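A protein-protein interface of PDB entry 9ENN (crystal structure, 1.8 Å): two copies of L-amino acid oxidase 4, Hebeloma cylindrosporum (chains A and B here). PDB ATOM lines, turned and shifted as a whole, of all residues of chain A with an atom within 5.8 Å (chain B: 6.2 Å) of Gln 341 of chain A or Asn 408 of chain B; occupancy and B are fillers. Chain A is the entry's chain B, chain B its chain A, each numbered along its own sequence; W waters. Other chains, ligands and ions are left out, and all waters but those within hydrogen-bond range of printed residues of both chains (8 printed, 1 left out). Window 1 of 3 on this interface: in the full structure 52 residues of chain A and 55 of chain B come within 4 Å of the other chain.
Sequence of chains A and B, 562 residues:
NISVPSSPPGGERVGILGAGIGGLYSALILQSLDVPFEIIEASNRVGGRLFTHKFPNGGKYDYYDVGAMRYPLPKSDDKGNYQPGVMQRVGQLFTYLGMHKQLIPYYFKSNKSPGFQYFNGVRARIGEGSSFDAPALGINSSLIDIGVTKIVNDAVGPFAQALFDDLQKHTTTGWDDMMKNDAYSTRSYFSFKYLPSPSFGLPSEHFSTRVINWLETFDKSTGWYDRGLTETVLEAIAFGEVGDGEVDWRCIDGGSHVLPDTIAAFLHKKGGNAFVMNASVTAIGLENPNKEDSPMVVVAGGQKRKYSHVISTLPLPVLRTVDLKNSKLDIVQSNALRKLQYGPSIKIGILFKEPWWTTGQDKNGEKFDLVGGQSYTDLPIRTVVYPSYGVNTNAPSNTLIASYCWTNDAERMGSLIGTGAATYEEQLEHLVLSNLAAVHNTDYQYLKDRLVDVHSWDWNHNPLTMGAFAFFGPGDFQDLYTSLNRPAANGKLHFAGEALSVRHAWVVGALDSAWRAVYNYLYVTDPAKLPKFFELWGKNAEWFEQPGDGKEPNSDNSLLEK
No position is printed for both chains.
Of the 15 printed residues of chain B, 5 touch a printed residue of chain A. Printed residues of chain A that touch a printed residue of chain B: Arg 338, Lys 339, Leu 340, Gln 341, Tyr 342, Gly 473 and Pro 474. Hydrophobic or aromatic side chains of chain A within 4 Å of the printed part of chain B: Tyr 342 and Pro 474. Among the printed residues, 9 pairs touch across the chains. Among the printed residues, no Asp or Glu carboxylate lies within 4 Å of a Lys or Arg side-chain nitrogen of the other chain.
Water W6 lies within hydrogen-bond range of OD2 of Asp 226 of chain B, NZ of Lys 339 of chain A and O of Pro 474 of chain A. Water W7 lies within hydrogen-bond range of OD1 of Asn 408 of chain B (2.6 Å) and NZ of Lys 339 of chain A (2.8 Å). Water W5 bridges the side-chain carboxylate of Glu 216 of chain B and the guanidinium group of Arg 338 of chain A. Water W4 lies within hydrogen-bond range of the side-chain carboxylate (OE1) of Glu 411 of chain B, the backbone carbonyl oxygen (O) of Tyr 342 of chain A and the guanidinium group (NH2) of Arg 227 of chain A. Water W8 bridges the side-chain amide nitrogen of Gln 341 of chain A (2.9 Å) and the side-chain carboxylate of Asp 226 of chain B (2.9 Å). Water W1 bridges the backbone carbonyl oxygen (O) of Arg 338 of chain A (2.9 Å) and the side-chain carboxylate (OD1) of Asp 409 of chain B (2.9 Å).
Among the printed residues, pairs that only touch across the chains: Lys 339 of chain A with Glu 216 of chain B (3.9 Å), Lys 339 of chain A with Thr 222 of chain B (3.9 Å), Tyr 342 of chain A with Arg 412 of chain B (3.9 Å), Gly 473 of chain A with Asp 226 of chain B (3.95 Å) and Pro 474 of chain A with Asp 226 of chain B (3.5 Å).
OG1 of Thr 222 of chain B sits at hydrogen-bond distance from NH1 of Arg 338 of chain A. The side-chain amide nitrogen of Asn 408 of chain B sits at hydrogen-bond distance from the side-chain amide oxygen of Gln 341 of chain A. The guanidinium group of Arg 412 of chain B is in hydrogen-bond range of the backbone carbonyl oxygen of Arg 338 of chain A, at 3.4 Å. The backbone carbonyl oxygen (O) of Leu 340 of chain A is in hydrogen-bond range of the guanidinium group (NH2) of Arg 412 of chain B (2.9 Å).
Of the printed residues of chain B, Arg 338 of chain A touches Thr 222 and Arg 412. Gln 341 of chain A touches just one residue of chain B: Asn 408 (3.0 Å). Of the printed residues of chain B, Tyr 342 of chain A touches Arg 412. Phe 471 of chain A touches none of the printed residues of chain B. Printed residues of chain B within 4 Å of Pro 474 of chain A: Asp 226 (3.5 Å). Of the printed residues of chain A, Glu 216 of chain B touches Lys 339 (3.9 Å). The nearest residue of chain A that does not touch Asn 408 of chain B is Lys 339 of chain A (4.7 Å).
The backbone carbonyl oxygen (O) of Thr 222 of chain B sits at hydrogen-bond distance from the side-chain hydroxyl (OG1) of Thr 407 of chain B, at 2.7 Å. O of Thr 222 of chain B sits at hydrogen-bond distance from N of Asn 408 of chain B (2.9 Å). The side-chain carboxylate (OE1) of Glu 411 of chain B is in hydrogen-bond range of the side-chain amide nitrogen (ND2) of Asn 408 of chain B (2.9 Å). The backbone carbonyl oxygen of Gln 341 of chain A is in hydrogen-bond range of the backbone NH of Phe 471 of chain A (2.8 Å). The side-chain amide nitrogen of Gln 341 of chain A lies close to the backbone NH of Gly 473 of chain A, 3.4 Å away. N of Gly 473 of chain A is in hydrogen-bond range of OD2 of Asp 476 of chain A (3.0 Å).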
ATOM      1  N   ARG A 227     -12.081   6.328  -7.446  1.00  0.00           N
ATOM      2  CA  ARG A 227     -11.925   7.133  -6.248  1.00  0.00           C
ATOM      3  C   ARG A 227     -10.776   6.568  -5.418  1.00  0.00           C
ATOM      4  O   ARG A 227     -10.099   5.620  -5.823  1.00  0.00           O
ATOM      5  CB  ARG A 227     -13.253   7.185  -5.503  1.00  0.00           C
ATOM      6  CG  ARG A 227     -14.334   7.638  -6.473  1.00  0.00           C
ATOM      7  CD  ARG A 227     -15.449   8.366  -5.822  1.00  0.00           C
ATOM      8  NE  ARG A 227     -16.356   8.938  -6.807  1.00  0.00           N
ATOM      9  CZ  ARG A 227     -16.948  10.112  -6.654  1.00  0.00           C
ATOM     10  NH1 ARG A 227     -16.678  10.887  -5.617  1.00  0.00           N
ATOM     11  NH2 ARG A 227     -17.829  10.521  -7.561  1.00  0.00           N
ATOM     12  N   GLU A 231     -10.561   5.093   0.544  1.00  0.00           N
ATOM     13  CA  GLU A 231     -11.996   4.945   0.770  1.00  0.00           C
ATOM     14  C   GLU A 231     -12.422   3.484   0.664  1.00  0.00           C
ATOM     15  O   GLU A 231     -13.257   3.021   1.448  1.00  0.00           O
ATOM     16  CB  GLU A 231     -12.794   5.801  -0.215  1.00  0.00           C
ATOM     17  CG  GLU A 231     -12.718   7.296   0.047  1.00  0.00           C
ATOM     18  CD  GLU A 231     -13.570   7.762   1.230  1.00  0.00           C
ATOM     19  OE1 GLU A 231     -13.735   7.019   2.224  1.00  0.00           O
ATOM     20  OE2 GLU A 231     -14.058   8.909   1.183  1.00  0.00           O
ATOM     21  N   ARG A 338     -13.247  23.105  -1.597  1.00  0.00           N
ATOM     22  CA  ARG A 338     -13.566  22.886  -3.005  1.00  0.00           C
ATOM     23  C   ARG A 338     -13.199  21.478  -3.468  1.00  0.00           C
ATOM     24  O   ARG A 338     -13.978  20.830  -4.177  1.00  0.00           O
ATOM     25  CB  ARG A 338     -12.841  23.919  -3.876  1.00  0.00           C
ATOM     26  CG  ARG A 338     -12.992  23.708  -5.378  1.00  0.00           C
ATOM     27  CD  ARG A 338     -12.263  24.808  -6.174  1.00  0.00           C
ATOM     28  NE  ARG A 338     -10.832  24.831  -5.879  1.00  0.00           N
ATOM     29  CZ  ARG A 338      -9.934  24.033  -6.444  1.00  0.00           C
ATOM     30  NH1 ARG A 338     -10.280  23.128  -7.345  1.00  0.00           N
ATOM     31  NH2 ARG A 338      -8.660  24.121  -6.073  1.00  0.00           N
ATOM     32  N   LYS A 339     -12.006  21.000  -3.107  1.00  0.00           N
ATOM     33  CA  LYS A 339     -11.440  19.806  -3.727  1.00  0.00           C
ATOM     34  C   LYS A 339     -11.841  18.512  -3.028  1.00  0.00           C
ATOM     35  O   LYS A 339     -11.982  17.488  -3.700  1.00  0.00           O
ATOM     36  CB  LYS A 339      -9.908  19.929  -3.782  1.00  0.00           C
ATOM     37  CG  LYS A 339      -9.148  18.670  -4.244  1.00  0.00           C
ATOM     38  CD  LYS A 339      -9.501  18.249  -5.667  1.00  0.00           C
ATOM     39  CE  LYS A 339      -8.935  16.871  -6.005  1.00  0.00           C
ATOM     40  NZ  LYS A 339      -9.670  15.783  -5.284  1.00  0.00           N
ATOM     41  N   LEU A 340     -12.027  18.501  -1.712  1.00  0.00           N
ATOM     42  CA  LEU A 340     -12.388  17.246  -1.054  1.00  0.00           C
ATOM     43  C   LEU A 340     -13.687  16.707  -1.658  1.00  0.00           C
ATOM     44  O   LEU A 340     -14.731  17.363  -1.593  1.00  0.00           O
ATOM     45  CB  LEU A 340     -12.523  17.458   0.450  1.00  0.00           C
ATOM     46  CG  LEU A 340     -11.209  17.716   1.199  1.00  0.00           C
ATOM     47  CD1 LEU A 340     -11.530  17.976   2.646  1.00  0.00           C
ATOM     48  CD2 LEU A 340     -10.230  16.551   1.058  1.00  0.00           C
ATOM     49  N   GLN A 341     -13.625  15.512  -2.248  1.00  0.00           N
ATOM     50  CA  GLN A 341     -14.654  15.082  -3.188  1.00  0.00           C
ATOM     51  C   GLN A 341     -15.868  14.438  -2.516  1.00  0.00           C
ATOM     52  O   GLN A 341     -15.745  13.681  -1.548  1.00  0.00           O
ATOM     53  CB  GLN A 341     -14.063  14.102  -4.213  1.00  0.00           C
ATOM     54  CG  GLN A 341     -14.974  13.885  -5.414  1.00  0.00           C
ATOM     55  CD  GLN A 341     -14.383  13.006  -6.503  1.00  0.00           C
ATOM     56  OE1 GLN A 341     -14.747  13.138  -7.669  1.00  0.00           O
ATOM     57  NE2 GLN A 341     -13.500  12.087  -6.129  1.00  0.00           N
ATOM     58  N   TYR A 342     -17.044  14.743  -3.065  1.00  0.00           N
ATOM     59  CA  TYR A 342     -18.316  14.131  -2.711  1.00  0.00           C
ATOM     60  C   TYR A 342     -18.725  13.110  -3.768  1.00  0.00           C
ATOM     61  O   TYR A 342     -18.257  13.141  -4.911  1.00  0.00           O
ATOM     62  CB  TYR A 342     -19.408  15.206  -2.559  1.00  0.00           C
ATOM     63  CG  TYR A 342     -19.429  15.779  -1.161  1.00  0.00           C
ATOM     64  CD1 TYR A 342     -18.291  16.366  -0.617  1.00  0.00           C
ATOM     65  CD2 TYR A 342     -20.560  15.682  -0.360  1.00  0.00           C
ATOM     66  CE1 TYR A 342     -18.281  16.857   0.693  1.00  0.00           C
ATOM     67  CE2 TYR A 342     -20.565  16.183   0.942  1.00  0.00           C
ATOM     68  CZ  TYR A 342     -19.422  16.771   1.466  1.00  0.00           C
ATOM     69  OH  TYR A 342     -19.418  17.260   2.763  1.00  0.00           O
ATOM     70  N   GLY A 343     -19.600  12.187  -3.358  1.00  0.00           N
ATOM     71  CA  GLY A 343     -20.176  11.202  -4.245  1.00  0.00           C
ATOM     72  C   GLY A 343     -21.693  11.274  -4.312  1.00  0.00           C
ATOM     73  O   GLY A 343     -22.359  11.779  -3.402  1.00  0.00           O
ATOM     74  N   PHE A 469     -22.729  12.291  -0.034  1.00  0.00           N
ATOM     75  CA  PHE A 469     -21.794  12.202   1.080  1.00  0.00           C
ATOM     76  C   PHE A 469     -20.380  12.347   0.541  1.00  0.00           C
ATOM     77  O   PHE A 469     -20.137  12.241  -0.666  1.00  0.00           O
ATOM     78  CB  PHE A 469     -21.927  10.873   1.866  1.00  0.00           C
ATOM     79  CG  PHE A 469     -22.322   9.688   1.017  1.00  0.00           C
ATOM     80  CD1 PHE A 469     -21.512   9.251  -0.015  1.00  0.00           C
ATOM     81  CD2 PHE A 469     -23.506   9.010   1.256  1.00  0.00           C
ATOM     82  CE1 PHE A 469     -21.878   8.171  -0.800  1.00  0.00           C
ATOM     83  CE2 PHE A 469     -23.880   7.930   0.469  1.00  0.00           C
ATOM     84  CZ  PHE A 469     -23.058   7.506  -0.554  1.00  0.00           C
ATOM     85  N   ALA A 470     -19.451  12.605   1.455  1.00  0.00           N
ATOM     86  CA  ALA A 470     -18.045  12.614   1.090  1.00  0.00           C
ATOM     87  C   ALA A 470     -17.653  11.263   0.506  1.00  0.00           C
ATOM     88  O   ALA A 470     -18.059  10.212   1.006  1.00  0.00           O
ATOM     89  CB  ALA A 470     -17.181  12.937   2.307  1.00  0.00           C
ATOM     90  N   PHE A 471     -16.878  11.302  -0.576  1.00  0.00           N
ATOM     91  CA  PHE A 471     -16.324  10.100  -1.208  1.00  0.00           C
ATOM     92  C   PHE A 471     -15.029  10.568  -1.880  1.00  0.00           C
ATOM     93  O   PHE A 471     -15.001  10.891  -3.072  1.00  0.00           O
ATOM     94  CB  PHE A 471     -17.311   9.463  -2.173  1.00  0.00           C
ATOM     95  CG  PHE A 471     -16.935   8.065  -2.622  1.00  0.00           C
ATOM     96  CD1 PHE A 471     -15.670   7.535  -2.379  1.00  0.00           C
ATOM     97  CD2 PHE A 471     -17.857   7.282  -3.304  1.00  0.00           C
ATOM     98  CE1 PHE A 471     -15.332   6.252  -2.807  1.00  0.00           C
ATOM     99  CE2 PHE A 471     -17.524   5.996  -3.734  1.00  0.00           C
ATOM    100  CZ  PHE A 471     -16.257   5.485  -3.483  1.00  0.00           C
ATOM    101  N   PHE A 472     -13.960  10.594  -1.083  1.00  0.00           N
ATOM    102  CA  PHE A 472     -12.740  11.292  -1.452  1.00  0.00           C
ATOM    103  C   PHE A 472     -12.045  10.631  -2.640  1.00  0.00           C
ATOM    104  O   PHE A 472     -12.030   9.403  -2.777  1.00  0.00           O
ATOM    105  CB  PHE A 472     -11.765  11.323  -0.262  1.00  0.00           C
ATOM    106  CG  PHE A 472     -12.108  12.325   0.829  1.00  0.00           C
ATOM    107  CD1 PHE A 472     -13.265  13.082   0.793  1.00  0.00           C
ATOM    108  CD2 PHE A 472     -11.237  12.512   1.897  1.00  0.00           C
ATOM    109  CE1 PHE A 472     -13.552  13.999   1.802  1.00  0.00           C
ATOM    110  CE2 PHE A 472     -11.520  13.423   2.909  1.00  0.00           C
ATOM    111  CZ  PHE A 472     -12.675  14.170   2.857  1.00  0.00           C
ATOM    112  N   GLY A 473     -11.454  11.458  -3.494  1.00  0.00           N
ATOM    113  CA  GLY A 473     -10.567  10.965  -4.518  1.00  0.00           C
ATOM    114  C   GLY A 473      -9.193  10.702  -3.950  1.00  0.00           C
ATOM    115  O   GLY A 473      -8.884  11.013  -2.791  1.00  0.00           O
ATOM    116  N   PRO A 474      -8.334  10.100  -4.764  1.00  0.00           N
ATOM    117  CA  PRO A 474      -6.951   9.874  -4.319  1.00  0.00           C
ATOM    118  C   PRO A 474      -6.275  11.185  -3.941  1.00  0.00           C
ATOM    119  O   PRO A 474      -6.434  12.199  -4.621  1.00  0.00           O
ATOM    120  CB  PRO A 474      -6.282   9.226  -5.537  1.00  0.00           C
ATOM    121  CG  PRO A 474      -7.400   8.722  -6.382  1.00  0.00           C
ATOM    122  CD  PRO A 474      -8.577   9.613  -6.134  1.00  0.00           C
ATOM    123  N   ASP A 476      -6.842  13.144  -1.400  1.00  0.00           N
ATOM    124  CA  ASP A 476      -7.638  14.021  -0.549  1.00  0.00           C
ATOM    125  C   ASP A 476      -7.298  13.824   0.929  1.00  0.00           C
ATOM    126  O   ASP A 476      -7.076  14.796   1.661  1.00  0.00           O
ATOM    127  CB  ASP A 476      -9.129  13.762  -0.800  1.00  0.00           C
ATOM    128  CG  ASP A 476      -9.665  14.435  -2.078  1.00  0.00           C
ATOM    129  OD1 ASP A 476      -8.967  15.272  -2.699  1.00  0.00           O
ATOM    130  OD2 ASP A 476     -10.826  14.142  -2.436  1.00  0.00           O
ATOM    131  N   GLU B 216      -3.963  20.962 -11.242  1.00  0.00           N
ATOM    132  CA  GLU B 216      -5.360  20.800 -11.643  1.00  0.00           C
ATOM    133  C   GLU B 216      -6.133  22.102 -11.471  1.00  0.00           C
ATOM    134  O   GLU B 216      -6.958  22.463 -12.318  1.00  0.00           O
ATOM    135  CB  GLU B 216      -6.038  19.681 -10.848  1.00  0.00           C
ATOM    136  CG  GLU B 216      -7.442  19.371 -11.371  1.00  0.00           C
ATOM    137  CD  GLU B 216      -8.218  18.390 -10.510  1.00  0.00           C
ATOM    138  OE1 GLU B 216      -8.696  18.796  -9.425  1.00  0.00           O
ATOM    139  OE2 GLU B 216      -8.388  17.227 -10.939  1.00  0.00           O
ATOM    140  N   SER B 221     -10.452  21.549 -14.221  1.00  0.00           N
ATOM    141  CA  SER B 221     -11.610  21.669 -13.342  1.00  0.00           C
ATOM    142  C   SER B 221     -11.425  20.702 -12.184  1.00  0.00           C
ATOM    143  O   SER B 221     -10.602  19.789 -12.250  1.00  0.00           O
ATOM    144  CB  SER B 221     -12.891  21.357 -14.126  1.00  0.00           C
ATOM    145  OG  SER B 221     -12.761  20.104 -14.782  1.00  0.00           O
ATOM    146  N   THR B 222     -12.181  20.907 -11.109  1.00  0.00           N
ATOM    147  CA  THR B 222     -12.009  20.081  -9.918  1.00  0.00           C
ATOM    148  C   THR B 222     -12.376  18.635 -10.229  1.00  0.00           C
ATOM    149  O   THR B 222     -13.524  18.349 -10.584  1.00  0.00           O
ATOM    150  CB  THR B 222     -12.874  20.610  -8.776  1.00  0.00           C
ATOM    151  OG1 THR B 222     -12.645  22.018  -8.623  1.00  0.00           O
ATOM    152  CG2 THR B 222     -12.578  19.880  -7.452  1.00  0.00           C
ATOM    153  N   GLY B 223     -11.408  17.726 -10.102  1.00  0.00           N
ATOM    154  CA  GLY B 223     -11.639  16.324 -10.362  1.00  0.00           C
ATOM    155  C   GLY B 223     -11.258  15.870 -11.752  1.00  0.00           C
ATOM    156  O   GLY B 223     -11.328  14.670 -12.035  1.00  0.00           O
ATOM    157  N   TRP B 224     -10.868  16.795 -12.628  1.00  0.00           N
ATOM    158  CA  TRP B 224     -10.475  16.411 -13.978  1.00  0.00           C
ATOM    159  C   TRP B 224      -9.390  15.342 -13.969  1.00  0.00           C
ATOM    160  O   TRP B 224      -9.431  14.395 -14.765  1.00  0.00           O
ATOM    161  CB  TRP B 224      -9.974  17.639 -14.737  1.00  0.00           C
ATOM    162  CG  TRP B 224      -9.527  17.351 -16.134  1.00  0.00           C
ATOM    163  CD1 TRP B 224      -8.423  16.641 -16.517  1.00  0.00           C
ATOM    164  CD2 TRP B 224     -10.164  17.781 -17.335  1.00  0.00           C
ATOM    165  NE1 TRP B 224      -8.339  16.605 -17.885  1.00  0.00           N
ATOM    166  CE2 TRP B 224      -9.401  17.291 -18.412  1.00  0.00           C
ATOM    167  CE3 TRP B 224     -11.309  18.534 -17.608  1.00  0.00           C
ATOM    168  CZ2 TRP B 224      -9.750  17.526 -19.738  1.00  0.00           C
ATOM    169  CZ3 TRP B 224     -11.654  18.763 -18.923  1.00  0.00           C
ATOM    170  CH2 TRP B 224     -10.877  18.262 -19.972  1.00  0.00           C
ATOM    171  N   ASP B 226      -8.662  12.941 -12.089  1.00  0.00           N
ATOM    172  CA  ASP B 226      -8.994  11.569 -11.724  1.00  0.00           C
ATOM    173  C   ASP B 226      -9.630  10.805 -12.882  1.00  0.00           C
ATOM    174  O   ASP B 226      -9.883   9.601 -12.762  1.00  0.00           O
ATOM    175  CB  ASP B 226      -9.907  11.549 -10.496  1.00  0.00           C
ATOM    176  CG  ASP B 226      -9.147  11.834  -9.195  1.00  0.00           C
ATOM    177  OD1 ASP B 226      -7.899  11.717  -9.154  1.00  0.00           O
ATOM    178  OD2 ASP B 226      -9.809  12.183  -8.199  1.00  0.00           O
ATOM    179  N   PRO B 344     -20.119  15.570 -16.339  1.00  0.00           N
ATOM    180  CA  PRO B 344     -21.184  16.567 -16.180  1.00  0.00           C
ATOM    181  C   PRO B 344     -20.763  17.942 -16.688  1.00  0.00           C
ATOM    182  O   PRO B 344     -19.583  18.221 -16.901  1.00  0.00           O
ATOM    183  CB  PRO B 344     -21.376  16.604 -14.656  1.00  0.00           C
ATOM    184  CG  PRO B 344     -19.904  16.468 -14.160  1.00  0.00           C
ATOM    185  CD  PRO B 344     -19.293  15.437 -15.118  1.00  0.00           C
ATOM    186  N   TRP B 406     -17.337  22.190 -15.171  1.00  0.00           N
ATOM    187  CA  TRP B 406     -17.129  20.777 -15.441  1.00  0.00           C
ATOM    188  C   TRP B 406     -16.980  19.980 -14.145  1.00  0.00           C
ATOM    189  O   TRP B 406     -16.874  20.536 -13.048  1.00  0.00           O
ATOM    190  CB  TRP B 406     -15.863  20.573 -16.284  1.00  0.00           C
ATOM    191  CG  TRP B 406     -15.879  21.201 -17.646  1.00  0.00           C
ATOM    192  CD1 TRP B 406     -16.964  21.413 -18.439  1.00  0.00           C
ATOM    193  CD2 TRP B 406     -14.740  21.670 -18.387  1.00  0.00           C
ATOM    194  NE1 TRP B 406     -16.577  21.993 -19.627  1.00  0.00           N
ATOM    195  CE2 TRP B 406     -15.216  22.156 -19.621  1.00  0.00           C
ATOM    196  CE3 TRP B 406     -13.367  21.727 -18.123  1.00  0.00           C
ATOM    197  CZ2 TRP B 406     -14.365  22.695 -20.593  1.00  0.00           C
ATOM    198  CZ3 TRP B 406     -12.519  22.251 -19.095  1.00  0.00           C
ATOM    199  CH2 TRP B 406     -13.022  22.730 -20.313  1.00  0.00           C
ATOM    200  N   THR B 407     -16.928  18.651 -14.310  1.00  0.00           N
ATOM    201  CA  THR B 407     -16.597  17.687 -13.261  1.00  0.00           C
ATOM    202  C   THR B 407     -17.217  18.060 -11.918  1.00  0.00           C
ATOM    203  O   THR B 407     -18.424  18.325 -11.865  1.00  0.00           O
ATOM    204  CB  THR B 407     -15.070  17.502 -13.192  1.00  0.00           C
ATOM    205  OG1 THR B 407     -14.373  18.746 -13.065  1.00  0.00           O
ATOM    206  CG2 THR B 407     -14.587  16.816 -14.496  1.00  0.00           C
ATOM    207  N   ASN B 408     -16.434  18.037 -10.829  1.00  0.00           N
ATOM    208  CA  ASN B 408     -17.037  18.210  -9.509  1.00  0.00           C
ATOM    209  C   ASN B 408     -17.707  19.577  -9.360  1.00  0.00           C
ATOM    210  O   ASN B 408     -18.669  19.719  -8.596  1.00  0.00           O
ATOM    211  CB  ASN B 408     -16.018  18.091  -8.366  1.00  0.00           C
ATOM    212  CG  ASN B 408     -15.357  16.726  -8.254  1.00  0.00           C
ATOM    213  OD1 ASN B 408     -14.237  16.639  -7.754  1.00  0.00           O
ATOM    214  ND2 ASN B 408     -16.049  15.665  -8.652  1.00  0.00           N
ATOM    215  N   ASP B 409     -17.159  20.611 -10.010  1.00  0.00           N
ATOM    216  CA  ASP B 409     -17.760  21.938  -9.905  1.00  0.00           C
ATOM    217  C   ASP B 409     -19.157  21.940 -10.511  1.00  0.00           C
ATOM    218  O   ASP B 409     -20.082  22.558  -9.969  1.00  0.00           O
ATOM    219  CB  ASP B 409     -16.878  22.972 -10.601  1.00  0.00           C
ATOM    220  CG  ASP B 409     -15.440  22.939 -10.115  1.00  0.00           C
ATOM    221  OD1 ASP B 409     -15.187  22.970  -8.884  1.00  0.00           O
ATOM    222  OD2 ASP B 409     -14.556  22.875 -10.990  1.00  0.00           O
ATOM    223  N   ALA B 410     -19.330  21.234 -11.630  1.00  0.00           N
ATOM    224  CA  ALA B 410     -20.651  21.114 -12.231  1.00  0.00           C
ATOM    225  C   ALA B 410     -21.567  20.238 -11.382  1.00  0.00           C
ATOM    226  O   ALA B 410     -22.764  20.525 -11.254  1.00  0.00           O
ATOM    227  CB  ALA B 410     -20.534  20.536 -13.639  1.00  0.00           C
ATOM    228  N   GLU B 411     -21.032  19.155 -10.811  1.00  0.00           N
ATOM    229  CA  GLU B 411     -21.850  18.290  -9.965  1.00  0.00           C
ATOM    230  C   GLU B 411     -22.442  19.076  -8.804  1.00  0.00           C
ATOM    231  O   GLU B 411     -23.650  19.008  -8.537  1.00  0.00           O
ATOM    232  CB  GLU B 411     -21.013  17.115  -9.455  1.00  0.00           C
ATOM    233  CG  GLU B 411     -20.728  16.109 -10.552  1.00  0.00           C
ATOM    234  CD  GLU B 411     -19.518  15.247 -10.305  1.00  0.00           C
ATOM    235  OE1 GLU B 411     -18.891  15.355  -9.227  1.00  0.00           O
ATOM    236  OE2 GLU B 411     -19.181  14.480 -11.233  1.00  0.00           O
ATOM    237  N   ARG B 412     -21.602  19.852  -8.120  1.00  0.00           N
ATOM    238  CA  ARG B 412     -22.069  20.626  -6.978  1.00  0.00           C
ATOM    239  C   ARG B 412     -23.045  21.714  -7.411  1.00  0.00           C
ATOM    240  O   ARG B 412     -24.123  21.852  -6.827  1.00  0.00           O
ATOM    241  CB  ARG B 412     -20.873  21.218  -6.237  1.00  0.00           C
ATOM    242  CG  ARG B 412     -19.977  20.176  -5.607  1.00  0.00           C
ATOM    243  CD  ARG B 412     -18.749  20.830  -5.028  1.00  0.00           C
ATOM    244  NE  ARG B 412     -17.995  19.912  -4.189  1.00  0.00           N
ATOM    245  CZ  ARG B 412     -17.226  20.290  -3.179  1.00  0.00           C
ATOM    246  NH1 ARG B 412     -17.068  21.567  -2.872  1.00  0.00           N
ATOM    247  NH2 ARG B 412     -16.632  19.362  -2.434  1.00  0.00           N
ATOM    248  N   MET B 413     -22.705  22.494  -8.440  1.00  0.00           N
ATOM    249  CA  MET B 413     -23.614  23.570  -8.830  1.00  0.00           C
ATOM    250  C   MET B 413     -24.961  23.026  -9.300  1.00  0.00           C
ATOM    251  O   MET B 413     -25.983  23.709  -9.173  1.00  0.00           O
ATOM    252  CB  MET B 413     -23.000  24.442  -9.926  1.00  0.00           C
ATOM    253  CG  MET B 413     -23.776  25.732 -10.187  1.00  0.00           C
ATOM    254  SD  MET B 413     -23.548  26.945  -8.875  1.00  0.00           S
ATOM    255  CE  MET B 413     -22.046  27.779  -9.396  1.00  0.00           C
HETATM  256  O   HOH W   1     -15.694  21.263  -6.535  1.00  0.00           O
HETATM  257  O   HOH W   2     -18.193  11.791 -10.776  1.00  0.00           O
HETATM  258  O   HOH W   3     -17.218  17.114  -4.826  1.00  0.00           O
HETATM  259  O   HOH W   4     -18.687  13.193  -7.616  1.00  0.00           O
HETATM  260  O   HOH W   5      -8.590  21.334  -8.766  1.00  0.00           O
HETATM  261  O   HOH W   6      -8.643  13.298  -6.150  1.00  0.00           O
HETATM  262  O   HOH W   7     -12.130  15.619  -6.596  1.00  0.00           O
HETATM  263  O   HOH W   8     -12.019  10.338  -7.886  1.00  0.00           O
